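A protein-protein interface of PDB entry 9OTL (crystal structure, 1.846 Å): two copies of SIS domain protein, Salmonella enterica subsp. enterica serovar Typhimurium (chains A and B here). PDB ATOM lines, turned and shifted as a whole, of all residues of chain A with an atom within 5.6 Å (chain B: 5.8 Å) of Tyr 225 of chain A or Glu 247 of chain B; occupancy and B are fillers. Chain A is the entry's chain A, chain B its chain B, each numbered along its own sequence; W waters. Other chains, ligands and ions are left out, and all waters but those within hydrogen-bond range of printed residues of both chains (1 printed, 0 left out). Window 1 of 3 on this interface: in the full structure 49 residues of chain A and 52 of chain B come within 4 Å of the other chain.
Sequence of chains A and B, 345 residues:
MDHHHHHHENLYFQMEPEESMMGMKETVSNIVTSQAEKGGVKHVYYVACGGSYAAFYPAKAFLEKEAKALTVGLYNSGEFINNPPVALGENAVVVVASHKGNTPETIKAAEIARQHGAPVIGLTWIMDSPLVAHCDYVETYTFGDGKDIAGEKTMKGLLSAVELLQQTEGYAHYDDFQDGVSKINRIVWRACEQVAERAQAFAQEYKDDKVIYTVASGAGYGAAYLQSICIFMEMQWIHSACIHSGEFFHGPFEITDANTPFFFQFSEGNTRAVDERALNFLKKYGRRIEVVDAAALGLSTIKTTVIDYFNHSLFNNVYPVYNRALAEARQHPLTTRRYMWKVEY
Position printed for both chains: 242. Of the 3 pairs that touch across the chains among the printed residues, none has its exchanged pair printed and touching as well.
Among the printed residues, pairs that only touch across the chains: Ile 229 of chain A with Pro 252 of chain B.
The side-chain hydroxyl (OH) of Tyr 225 of chain A is in hydrogen-bond range of the side-chain carboxylate (OE2) of Glu 247 of chain B (3.4 Å). ND1 of His 239 of chain A is in hydrogen-bond range of OE2 of Glu 254 of chain B (2.7 Å).
The side-chain sulfur (SG) of Cys 242 of chain A lies within hydrogen-bond range of the backbone NH (N) of Tyr 225 of chain A, at 3.5 Å. A ring nitrogen (NE2) of His 239 of chain A is in hydrogen-bond range of the side-chain hydroxyl of Ser 228 of chain A. N of His 244 of chain B sits at hydrogen-bond distance from OE1 of Glu 247 of chain B.
Printed residues of chain B within 4 Å of Ile 229 of chain A: Pro 252 (3.5 Å). Of the printed residues of chain B, His 239 of chain A touches Glu 254 (2.7 Å). Glu 247 of chain B touches just one residue of chain A: Tyr 225. Of the printed residues of chain A, Pro 252 of chain B touches Ile 229 (3.5 Å). Printed residues of chain A within 4 Å of Glu 254 of chain B: His 239 (2.7 Å). The nearest residue of chain A that does not touch Glu 247 of chain B is Asn 76 of chain A (5.1 Å).
Water W1 lies within hydrogen-bond range of the side-chain carboxylate of Glu 247 of chain B (2.7 Å) and the side-chain hydroxyl of Tyr 225 of chain A (2.8 Å).
Of the 15 printed residues of chain A, 3 touch a printed residue of chain B. Printed residues of chain A that touch a printed residue of chain B: Tyr 225, Ile 229 and His 239. Along chain A the printed residues that touch a printed residue of chain B span positions 225 to 239. Among the printed residues, no Asp or Glu carboxylate lies within 4 Å of a Lys or Arg side-chain nitrogen of the other chain.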
ATOM      1  N   ALA A  54     -32.008 -14.158 -12.160  1.00  0.00           N
ATOM      2  CA  ALA A  54     -32.096 -15.320 -13.048  1.00  0.00           C
ATOM      3  C   ALA A  54     -32.556 -16.555 -12.288  1.00  0.00           C
ATOM      4  O   ALA A  54     -33.298 -17.338 -12.829  1.00  0.00           O
ATOM      5  CB  ALA A  54     -30.764 -15.577 -13.686  1.00  0.00           C
ATOM      6  N   ASN A  76     -35.807  -6.763 -11.249  1.00  0.00           N
ATOM      7  CA  ASN A  76     -34.514  -6.346 -10.734  1.00  0.00           C
ATOM      8  C   ASN A  76     -34.776  -5.316  -9.632  1.00  0.00           C
ATOM      9  O   ASN A  76     -35.728  -4.562  -9.709  1.00  0.00           O
ATOM     10  CB  ASN A  76     -33.580  -5.991 -11.874  1.00  0.00           C
ATOM     11  CG  ASN A  76     -32.733  -4.786 -11.566  1.00  0.00           C
ATOM     12  OD1 ASN A  76     -33.261  -3.662 -11.525  1.00  0.00           O
ATOM     13  ND2 ASN A  76     -31.433  -4.995 -11.358  1.00  0.00           N
ATOM     14  N   THR A 214     -26.215 -18.425 -26.826  1.00  0.00           N
ATOM     15  CA  THR A 214     -27.008 -19.396 -26.103  1.00  0.00           C
ATOM     16  C   THR A 214     -28.436 -19.343 -26.604  1.00  0.00           C
ATOM     17  O   THR A 214     -28.956 -18.324 -27.035  1.00  0.00           O
ATOM     18  CB  THR A 214     -26.998 -19.132 -24.596  1.00  0.00           C
ATOM     19  OG1 THR A 214     -27.357 -17.761 -24.577  1.00  0.00           O
ATOM     20  CG2 THR A 214     -25.641 -19.321 -23.955  1.00  0.00           C
ATOM     21  N   TYR A 221     -35.110 -20.777 -18.965  1.00  0.00           N
ATOM     22  CA  TYR A 221     -34.446 -19.768 -19.773  1.00  0.00           C
ATOM     23  C   TYR A 221     -33.405 -19.047 -18.906  1.00  0.00           C
ATOM     24  O   TYR A 221     -32.337 -18.717 -19.403  1.00  0.00           O
ATOM     25  CB  TYR A 221     -35.487 -18.819 -20.350  1.00  0.00           C
ATOM     26  CG  TYR A 221     -34.819 -17.672 -21.072  1.00  0.00           C
ATOM     27  CD1 TYR A 221     -34.408 -17.832 -22.384  1.00  0.00           C
ATOM     28  CD2 TYR A 221     -34.552 -16.462 -20.431  1.00  0.00           C
ATOM     29  CE1 TYR A 221     -33.763 -16.816 -23.067  1.00  0.00           C
ATOM     30  CE2 TYR A 221     -33.933 -15.422 -21.118  1.00  0.00           C
ATOM     31  CZ  TYR A 221     -33.521 -15.610 -22.428  1.00  0.00           C
ATOM     32  OH  TYR A 221     -32.842 -14.663 -23.141  1.00  0.00           O
ATOM     33  N   GLY A 222     -33.746 -18.808 -17.631  1.00  0.00           N
ATOM     34  CA  GLY A 222     -32.855 -18.209 -16.656  1.00  0.00           C
ATOM     35  C   GLY A 222     -31.473 -18.832 -16.606  1.00  0.00           C
ATOM     36  O   GLY A 222     -30.456 -18.139 -16.419  1.00  0.00           O
ATOM     37  N   ALA A 223     -31.404 -20.153 -16.804  1.00  0.00           N
ATOM     38  CA  ALA A 223     -30.129 -20.836 -16.696  1.00  0.00           C
ATOM     39  C   ALA A 223     -29.327 -20.557 -17.960  1.00  0.00           C
ATOM     40  O   ALA A 223     -28.113 -20.434 -17.904  1.00  0.00           O
ATOM     41  CB  ALA A 223     -30.252 -22.354 -16.452  1.00  0.00           C
ATOM     42  N   ALA A 224     -30.004 -20.461 -19.101  1.00  0.00           N
ATOM     43  CA  ALA A 224     -29.283 -20.137 -20.313  1.00  0.00           C
ATOM     44  C   ALA A 224     -28.734 -18.698 -20.283  1.00  0.00           C
ATOM     45  O   ALA A 224     -27.620 -18.441 -20.739  1.00  0.00           O
ATOM     46  CB  ALA A 224     -30.185 -20.354 -21.483  1.00  0.00           C
ATOM     47  N   TYR A 225     -29.547 -17.766 -19.825  1.00  0.00           N
ATOM     48  CA  TYR A 225     -29.148 -16.379 -19.589  1.00  0.00           C
ATOM     49  C   TYR A 225     -27.879 -16.299 -18.741  1.00  0.00           C
ATOM     50  O   TYR A 225     -26.877 -15.634 -19.077  1.00  0.00           O
ATOM     51  CB  TYR A 225     -30.316 -15.629 -18.901  1.00  0.00           C
ATOM     52  CG  TYR A 225     -29.922 -14.167 -18.745  1.00  0.00           C
ATOM     53  CD1 TYR A 225     -29.815 -13.370 -19.872  1.00  0.00           C
ATOM     54  CD2 TYR A 225     -29.502 -13.643 -17.530  1.00  0.00           C
ATOM     55  CE1 TYR A 225     -29.372 -12.065 -19.799  1.00  0.00           C
ATOM     56  CE2 TYR A 225     -29.070 -12.330 -17.436  1.00  0.00           C
ATOM     57  CZ  TYR A 225     -28.996 -11.545 -18.578  1.00  0.00           C
ATOM     58  OH  TYR A 225     -28.571 -10.247 -18.559  1.00  0.00           O
ATOM     59  N   LEU A 226     -27.899 -17.014 -17.621  1.00  0.00           N
ATOM     60  CA  LEU A 226     -26.748 -17.038 -16.740  1.00  0.00           C
ATOM     61  C   LEU A 226     -25.579 -17.669 -17.458  1.00  0.00           C
ATOM     62  O   LEU A 226     -24.474 -17.221 -17.278  1.00  0.00           O
ATOM     63  CB  LEU A 226     -27.011 -17.763 -15.426  1.00  0.00           C
ATOM     64  CG  LEU A 226     -27.913 -17.071 -14.415  1.00  0.00           C
ATOM     65  CD1 LEU A 226     -28.220 -18.030 -13.266  1.00  0.00           C
ATOM     66  CD2 LEU A 226     -27.248 -15.819 -13.890  1.00  0.00           C
ATOM     67  N   GLN A 227     -25.792 -18.725 -18.254  1.00  0.00           N
ATOM     68  CA  GLN A 227     -24.696 -19.271 -19.028  1.00  0.00           C
ATOM     69  C   GLN A 227     -24.107 -18.295 -20.075  1.00  0.00           C
ATOM     70  O   GLN A 227     -22.922 -18.357 -20.391  1.00  0.00           O
ATOM     71  CB  GLN A 227     -25.207 -20.574 -19.628  1.00  0.00           C
ATOM     72  CG  GLN A 227     -24.222 -21.313 -20.516  1.00  0.00           C
ATOM     73  CD  GLN A 227     -22.977 -21.782 -19.778  1.00  0.00           C
ATOM     74  OE1 GLN A 227     -22.721 -21.541 -18.593  1.00  0.00           O
ATOM     75  NE2 GLN A 227     -22.108 -22.393 -20.548  1.00  0.00           N
ATOM     76  N   SER A 228     -24.950 -17.465 -20.680  1.00  0.00           N
ATOM     77  CA  SER A 228     -24.544 -16.415 -21.604  1.00  0.00           C
ATOM     78  C   SER A 228     -23.498 -15.529 -20.943  1.00  0.00           C
ATOM     79  O   SER A 228     -22.427 -15.282 -21.477  1.00  0.00           O
ATOM     80  CB  SER A 228     -25.766 -15.615 -21.977  1.00  0.00           C
ATOM     81  OG  SER A 228     -25.431 -14.537 -22.814  1.00  0.00           O
ATOM     82  N   ILE A 229     -23.764 -15.185 -19.700  1.00  0.00           N
ATOM     83  CA  ILE A 229     -22.856 -14.383 -18.894  1.00  0.00           C
ATOM     84  C   ILE A 229     -21.570 -15.142 -18.555  1.00  0.00           C
ATOM     85  O   ILE A 229     -20.495 -14.564 -18.652  1.00  0.00           O
ATOM     86  CB  ILE A 229     -23.615 -13.907 -17.661  1.00  0.00           C
ATOM     87  CG1 ILE A 229     -24.612 -12.863 -18.086  1.00  0.00           C
ATOM     88  CG2 ILE A 229     -22.692 -13.356 -16.569  1.00  0.00           C
ATOM     89  CD1 ILE A 229     -25.645 -12.627 -16.998  1.00  0.00           C
ATOM     90  N   CYS A 230     -21.646 -16.445 -18.233  1.00  0.00           N
ATOM     91  CA  CYS A 230     -20.443 -17.216 -17.981  1.00  0.00           C
ATOM     92  C   CYS A 230     -19.558 -17.354 -19.210  1.00  0.00           C
ATOM     93  O   CYS A 230     -18.350 -17.270 -19.099  1.00  0.00           O
ATOM     94  CB  CYS A 230     -20.736 -18.628 -17.450  1.00  0.00           C
ATOM     95  SG  CYS A 230     -21.488 -18.581 -15.806  1.00  0.00           S
ATOM     96  N   HIS A 239     -20.630  -9.593 -25.455  1.00  0.00           N
ATOM     97  CA  HIS A 239     -21.786 -10.248 -24.852  1.00  0.00           C
ATOM     98  C   HIS A 239     -22.906 -10.365 -25.882  1.00  0.00           C
ATOM     99  O   HIS A 239     -23.522  -9.360 -26.284  1.00  0.00           O
ATOM    100  CB  HIS A 239     -22.093  -9.601 -23.515  1.00  0.00           C
ATOM    101  CG  HIS A 239     -23.201 -10.256 -22.813  1.00  0.00           C
ATOM    102  ND1 HIS A 239     -24.102  -9.571 -22.036  1.00  0.00           N
ATOM    103  CD2 HIS A 239     -23.610 -11.539 -22.844  1.00  0.00           C
ATOM    104  CE1 HIS A 239     -25.006 -10.432 -21.595  1.00  0.00           C
ATOM    105  NE2 HIS A 239     -24.729 -11.614 -22.093  1.00  0.00           N
ATOM    106  N   CYS A 242     -28.856 -13.958 -25.804  1.00  0.00           N
ATOM    107  CA  CYS A 242     -29.340 -15.238 -25.317  1.00  0.00           C
ATOM    108  C   CYS A 242     -30.692 -15.416 -25.993  1.00  0.00           C
ATOM    109  O   CYS A 242     -31.641 -14.732 -25.639  1.00  0.00           O
ATOM    110  CB  CYS A 242     -29.429 -15.181 -23.786  1.00  0.00           C
ATOM    111  SG  CYS A 242     -30.079 -16.710 -23.079  1.00  0.00           S
ATOM    112  N   CYS B 242     -29.000  -6.600 -25.545  1.00  0.00           N
ATOM    113  CA  CYS B 242     -29.754  -5.410 -25.223  1.00  0.00           C
ATOM    114  C   CYS B 242     -29.803  -5.332 -23.698  1.00  0.00           C
ATOM    115  O   CYS B 242     -30.566  -6.067 -23.089  1.00  0.00           O
ATOM    116  CB  CYS B 242     -31.133  -5.563 -25.838  1.00  0.00           C
ATOM    117  SG  CYS B 242     -32.146  -4.089 -25.601  1.00  0.00           S
ATOM    118  N   ILE B 243     -28.949  -4.491 -23.116  1.00  0.00           N
ATOM    119  CA  ILE B 243     -28.655  -4.459 -21.692  1.00  0.00           C
ATOM    120  C   ILE B 243     -29.699  -3.593 -20.974  1.00  0.00           C
ATOM    121  O   ILE B 243     -29.939  -2.431 -21.348  1.00  0.00           O
ATOM    122  CB  ILE B 243     -27.237  -3.881 -21.544  1.00  0.00           C
ATOM    123  CG1 ILE B 243     -26.253  -4.640 -22.442  1.00  0.00           C
ATOM    124  CG2 ILE B 243     -26.754  -3.819 -20.095  1.00  0.00           C
ATOM    125  CD1 ILE B 243     -24.966  -3.887 -22.700  1.00  0.00           C
ATOM    126  N   HIS B 244     -30.297  -4.156 -19.932  1.00  0.00           N
ATOM    127  CA  HIS B 244     -31.068  -3.401 -18.964  1.00  0.00           C
ATOM    128  C   HIS B 244     -30.108  -2.528 -18.164  1.00  0.00           C
ATOM    129  O   HIS B 244     -29.062  -2.997 -17.766  1.00  0.00           O
ATOM    130  CB  HIS B 244     -31.878  -4.314 -18.033  1.00  0.00           C
ATOM    131  CG  HIS B 244     -33.065  -4.965 -18.649  1.00  0.00           C
ATOM    132  ND1 HIS B 244     -33.044  -6.177 -19.324  1.00  0.00           N
ATOM    133  CD2 HIS B 244     -34.350  -4.568 -18.635  1.00  0.00           C
ATOM    134  CE1 HIS B 244     -34.271  -6.482 -19.717  1.00  0.00           C
ATOM    135  NE2 HIS B 244     -35.085  -5.518 -19.323  1.00  0.00           N
ATOM    136  N   SER B 245     -30.477  -1.247 -17.962  1.00  0.00           N
ATOM    137  CA  SER B 245     -29.579  -0.279 -17.402  1.00  0.00           C
ATOM    138  C   SER B 245     -29.074  -0.725 -16.037  1.00  0.00           C
ATOM    139  O   SER B 245     -27.928  -0.442 -15.691  1.00  0.00           O
ATOM    140  CB  SER B 245     -30.252   1.080 -17.289  1.00  0.00           C
ATOM    141  OG  SER B 245     -30.639   1.538 -18.572  1.00  0.00           O
ATOM    142  N   GLY B 246     -29.944  -1.353 -15.255  1.00  0.00           N
ATOM    143  CA  GLY B 246     -29.573  -1.718 -13.894  1.00  0.00           C
ATOM    144  C   GLY B 246     -28.463  -2.769 -13.833  1.00  0.00           C
ATOM    145  O   GLY B 246     -27.805  -2.930 -12.794  1.00  0.00           O
ATOM    146  N   GLU B 247     -28.210  -3.469 -14.941  1.00  0.00           N
ATOM    147  CA  GLU B 247     -27.409  -4.665 -14.824  1.00  0.00           C
ATOM    148  C   GLU B 247     -25.918  -4.346 -14.924  1.00  0.00           C
ATOM    149  O   GLU B 247     -25.140  -5.202 -14.529  1.00  0.00           O
ATOM    150  CB  GLU B 247     -28.129  -5.772 -15.606  1.00  0.00           C
ATOM    151  CG  GLU B 247     -27.821  -5.869 -17.088  1.00  0.00           C
ATOM    152  CD  GLU B 247     -28.870  -6.725 -17.797  1.00  0.00           C
ATOM    153  OE1 GLU B 247     -28.856  -6.780 -19.034  1.00  0.00           O
ATOM    154  OE2 GLU B 247     -29.709  -7.359 -17.106  1.00  0.00           O
ATOM    155  N   PHE B 248     -25.519  -3.092 -15.274  1.00  0.00           N
ATOM    156  CA  PHE B 248     -24.135  -2.675 -15.227  1.00  0.00           C
ATOM    157  C   PHE B 248     -23.559  -2.746 -13.819  1.00  0.00           C
ATOM    158  O   PHE B 248     -22.334  -2.820 -13.640  1.00  0.00           O
ATOM    159  CB  PHE B 248     -23.913  -1.214 -15.678  1.00  0.00           C
ATOM    160  CG  PHE B 248     -23.992  -1.088 -17.187  1.00  0.00           C
ATOM    161  CD1 PHE B 248     -23.077  -1.749 -17.974  1.00  0.00           C
ATOM    162  CD2 PHE B 248     -25.016  -0.396 -17.803  1.00  0.00           C
ATOM    163  CE1 PHE B 248     -23.183  -1.776 -19.331  1.00  0.00           C
ATOM    164  CE2 PHE B 248     -25.121  -0.397 -19.186  1.00  0.00           C
ATOM    165  CZ  PHE B 248     -24.197  -1.075 -19.952  1.00  0.00           C
ATOM    166  N   PHE B 249     -24.408  -2.624 -12.802  1.00  0.00           N
ATOM    167  CA  PHE B 249     -23.903  -2.447 -11.447  1.00  0.00           C
ATOM    168  C   PHE B 249     -23.727  -3.802 -10.822  1.00  0.00           C
ATOM    169  O   PHE B 249     -23.419  -3.900  -9.646  1.00  0.00           O
ATOM    170  CB  PHE B 249     -24.832  -1.594 -10.570  1.00  0.00           C
ATOM    171  CG  PHE B 249     -25.149  -0.386 -11.429  1.00  0.00           C
ATOM    172  CD1 PHE B 249     -24.142   0.488 -11.784  1.00  0.00           C
ATOM    173  CD2 PHE B 249     -26.392  -0.251 -12.017  1.00  0.00           C
ATOM    174  CE1 PHE B 249     -24.407   1.530 -12.665  1.00  0.00           C
ATOM    175  CE2 PHE B 249     -26.642   0.776 -12.904  1.00  0.00           C
ATOM    176  CZ  PHE B 249     -25.646   1.640 -13.245  1.00  0.00           C
ATOM    177  N   HIS B 250     -23.990  -4.855 -11.578  1.00  0.00           N
ATOM    178  CA  HIS B 250     -23.883  -6.142 -10.930  1.00  0.00           C
ATOM    179  C   HIS B 250     -23.117  -7.070 -11.852  1.00  0.00           C
ATOM    180  O   HIS B 250     -23.367  -7.115 -13.062  1.00  0.00           O
ATOM    181  CB  HIS B 250     -25.272  -6.681 -10.563  1.00  0.00           C
ATOM    182  CG  HIS B 250     -26.079  -5.726  -9.790  1.00  0.00           C
ATOM    183  ND1 HIS B 250     -25.884  -5.487  -8.443  1.00  0.00           N
ATOM    184  CD2 HIS B 250     -27.049  -4.872 -10.202  1.00  0.00           C
ATOM    185  CE1 HIS B 250     -26.736  -4.553  -8.044  1.00  0.00           C
ATOM    186  NE2 HIS B 250     -27.446  -4.161  -9.096  1.00  0.00           N
ATOM    187  N   GLY B 251     -22.194  -7.804 -11.235  1.00  0.00           N
ATOM    188  CA  GLY B 251     -21.486  -8.857 -11.921  1.00  0.00           C
ATOM    189  C   GLY B 251     -20.666  -8.276 -13.057  1.00  0.00           C
ATOM    190  O   GLY B 251     -20.241  -7.129 -13.016  1.00  0.00           O
ATOM    191  N   PRO B 252     -20.446  -9.054 -14.123  1.00  0.00           N
ATOM    192  CA  PRO B 252     -19.680  -8.544 -15.253  1.00  0.00           C
ATOM    193  C   PRO B 252     -20.377  -7.377 -15.966  1.00  0.00           C
ATOM    194  O   PRO B 252     -21.568  -7.225 -15.867  1.00  0.00           O
ATOM    195  CB  PRO B 252     -19.600  -9.723 -16.200  1.00  0.00           C
ATOM    196  CG  PRO B 252     -20.641 -10.710 -15.689  1.00  0.00           C
ATOM    197  CD  PRO B 252     -20.903 -10.449 -14.256  1.00  0.00           C
ATOM    198  N   PHE B 253     -19.632  -6.628 -16.754  1.00  0.00           N
ATOM    199  CA  PHE B 253     -20.220  -5.607 -17.601  1.00  0.00           C
ATOM    200  C   PHE B 253     -19.474  -5.587 -18.916  1.00  0.00           C
ATOM    201  O   PHE B 253     -18.297  -5.968 -18.977  1.00  0.00           O
ATOM    202  CB  PHE B 253     -20.223  -4.240 -16.922  1.00  0.00           C
ATOM    203  CG  PHE B 253     -18.928  -3.854 -16.228  1.00  0.00           C
ATOM    204  CD1 PHE B 253     -18.731  -4.141 -14.877  1.00  0.00           C
ATOM    205  CD2 PHE B 253     -17.948  -3.118 -16.881  1.00  0.00           C
ATOM    206  CE1 PHE B 253     -17.530  -3.818 -14.248  1.00  0.00           C
ATOM    207  CE2 PHE B 253     -16.763  -2.757 -16.226  1.00  0.00           C
ATOM    208  CZ  PHE B 253     -16.562  -3.116 -14.912  1.00  0.00           C
ATOM    209  N   GLU B 254     -20.152  -5.009 -19.918  1.00  0.00           N
ATOM    210  CA  GLU B 254     -19.803  -5.179 -21.313  1.00  0.00           C
ATOM    211  C   GLU B 254     -18.721  -4.187 -21.758  1.00  0.00           C
ATOM    212  O   GLU B 254     -18.883  -3.462 -22.743  1.00  0.00           O
ATOM    213  CB  GLU B 254     -21.072  -5.034 -22.142  1.00  0.00           C
ATOM    214  CG  GLU B 254     -22.096  -6.155 -21.969  1.00  0.00           C
ATOM    215  CD  GLU B 254     -23.009  -6.207 -20.750  1.00  0.00           C
ATOM    216  OE1 GLU B 254     -22.876  -5.351 -19.832  1.00  0.00           O
ATOM    217  OE2 GLU B 254     -23.822  -7.198 -20.696  1.00  0.00           O
HETATM  218  O   HOH W   1     -27.994  -8.671 -20.764  1.00  0.00           O
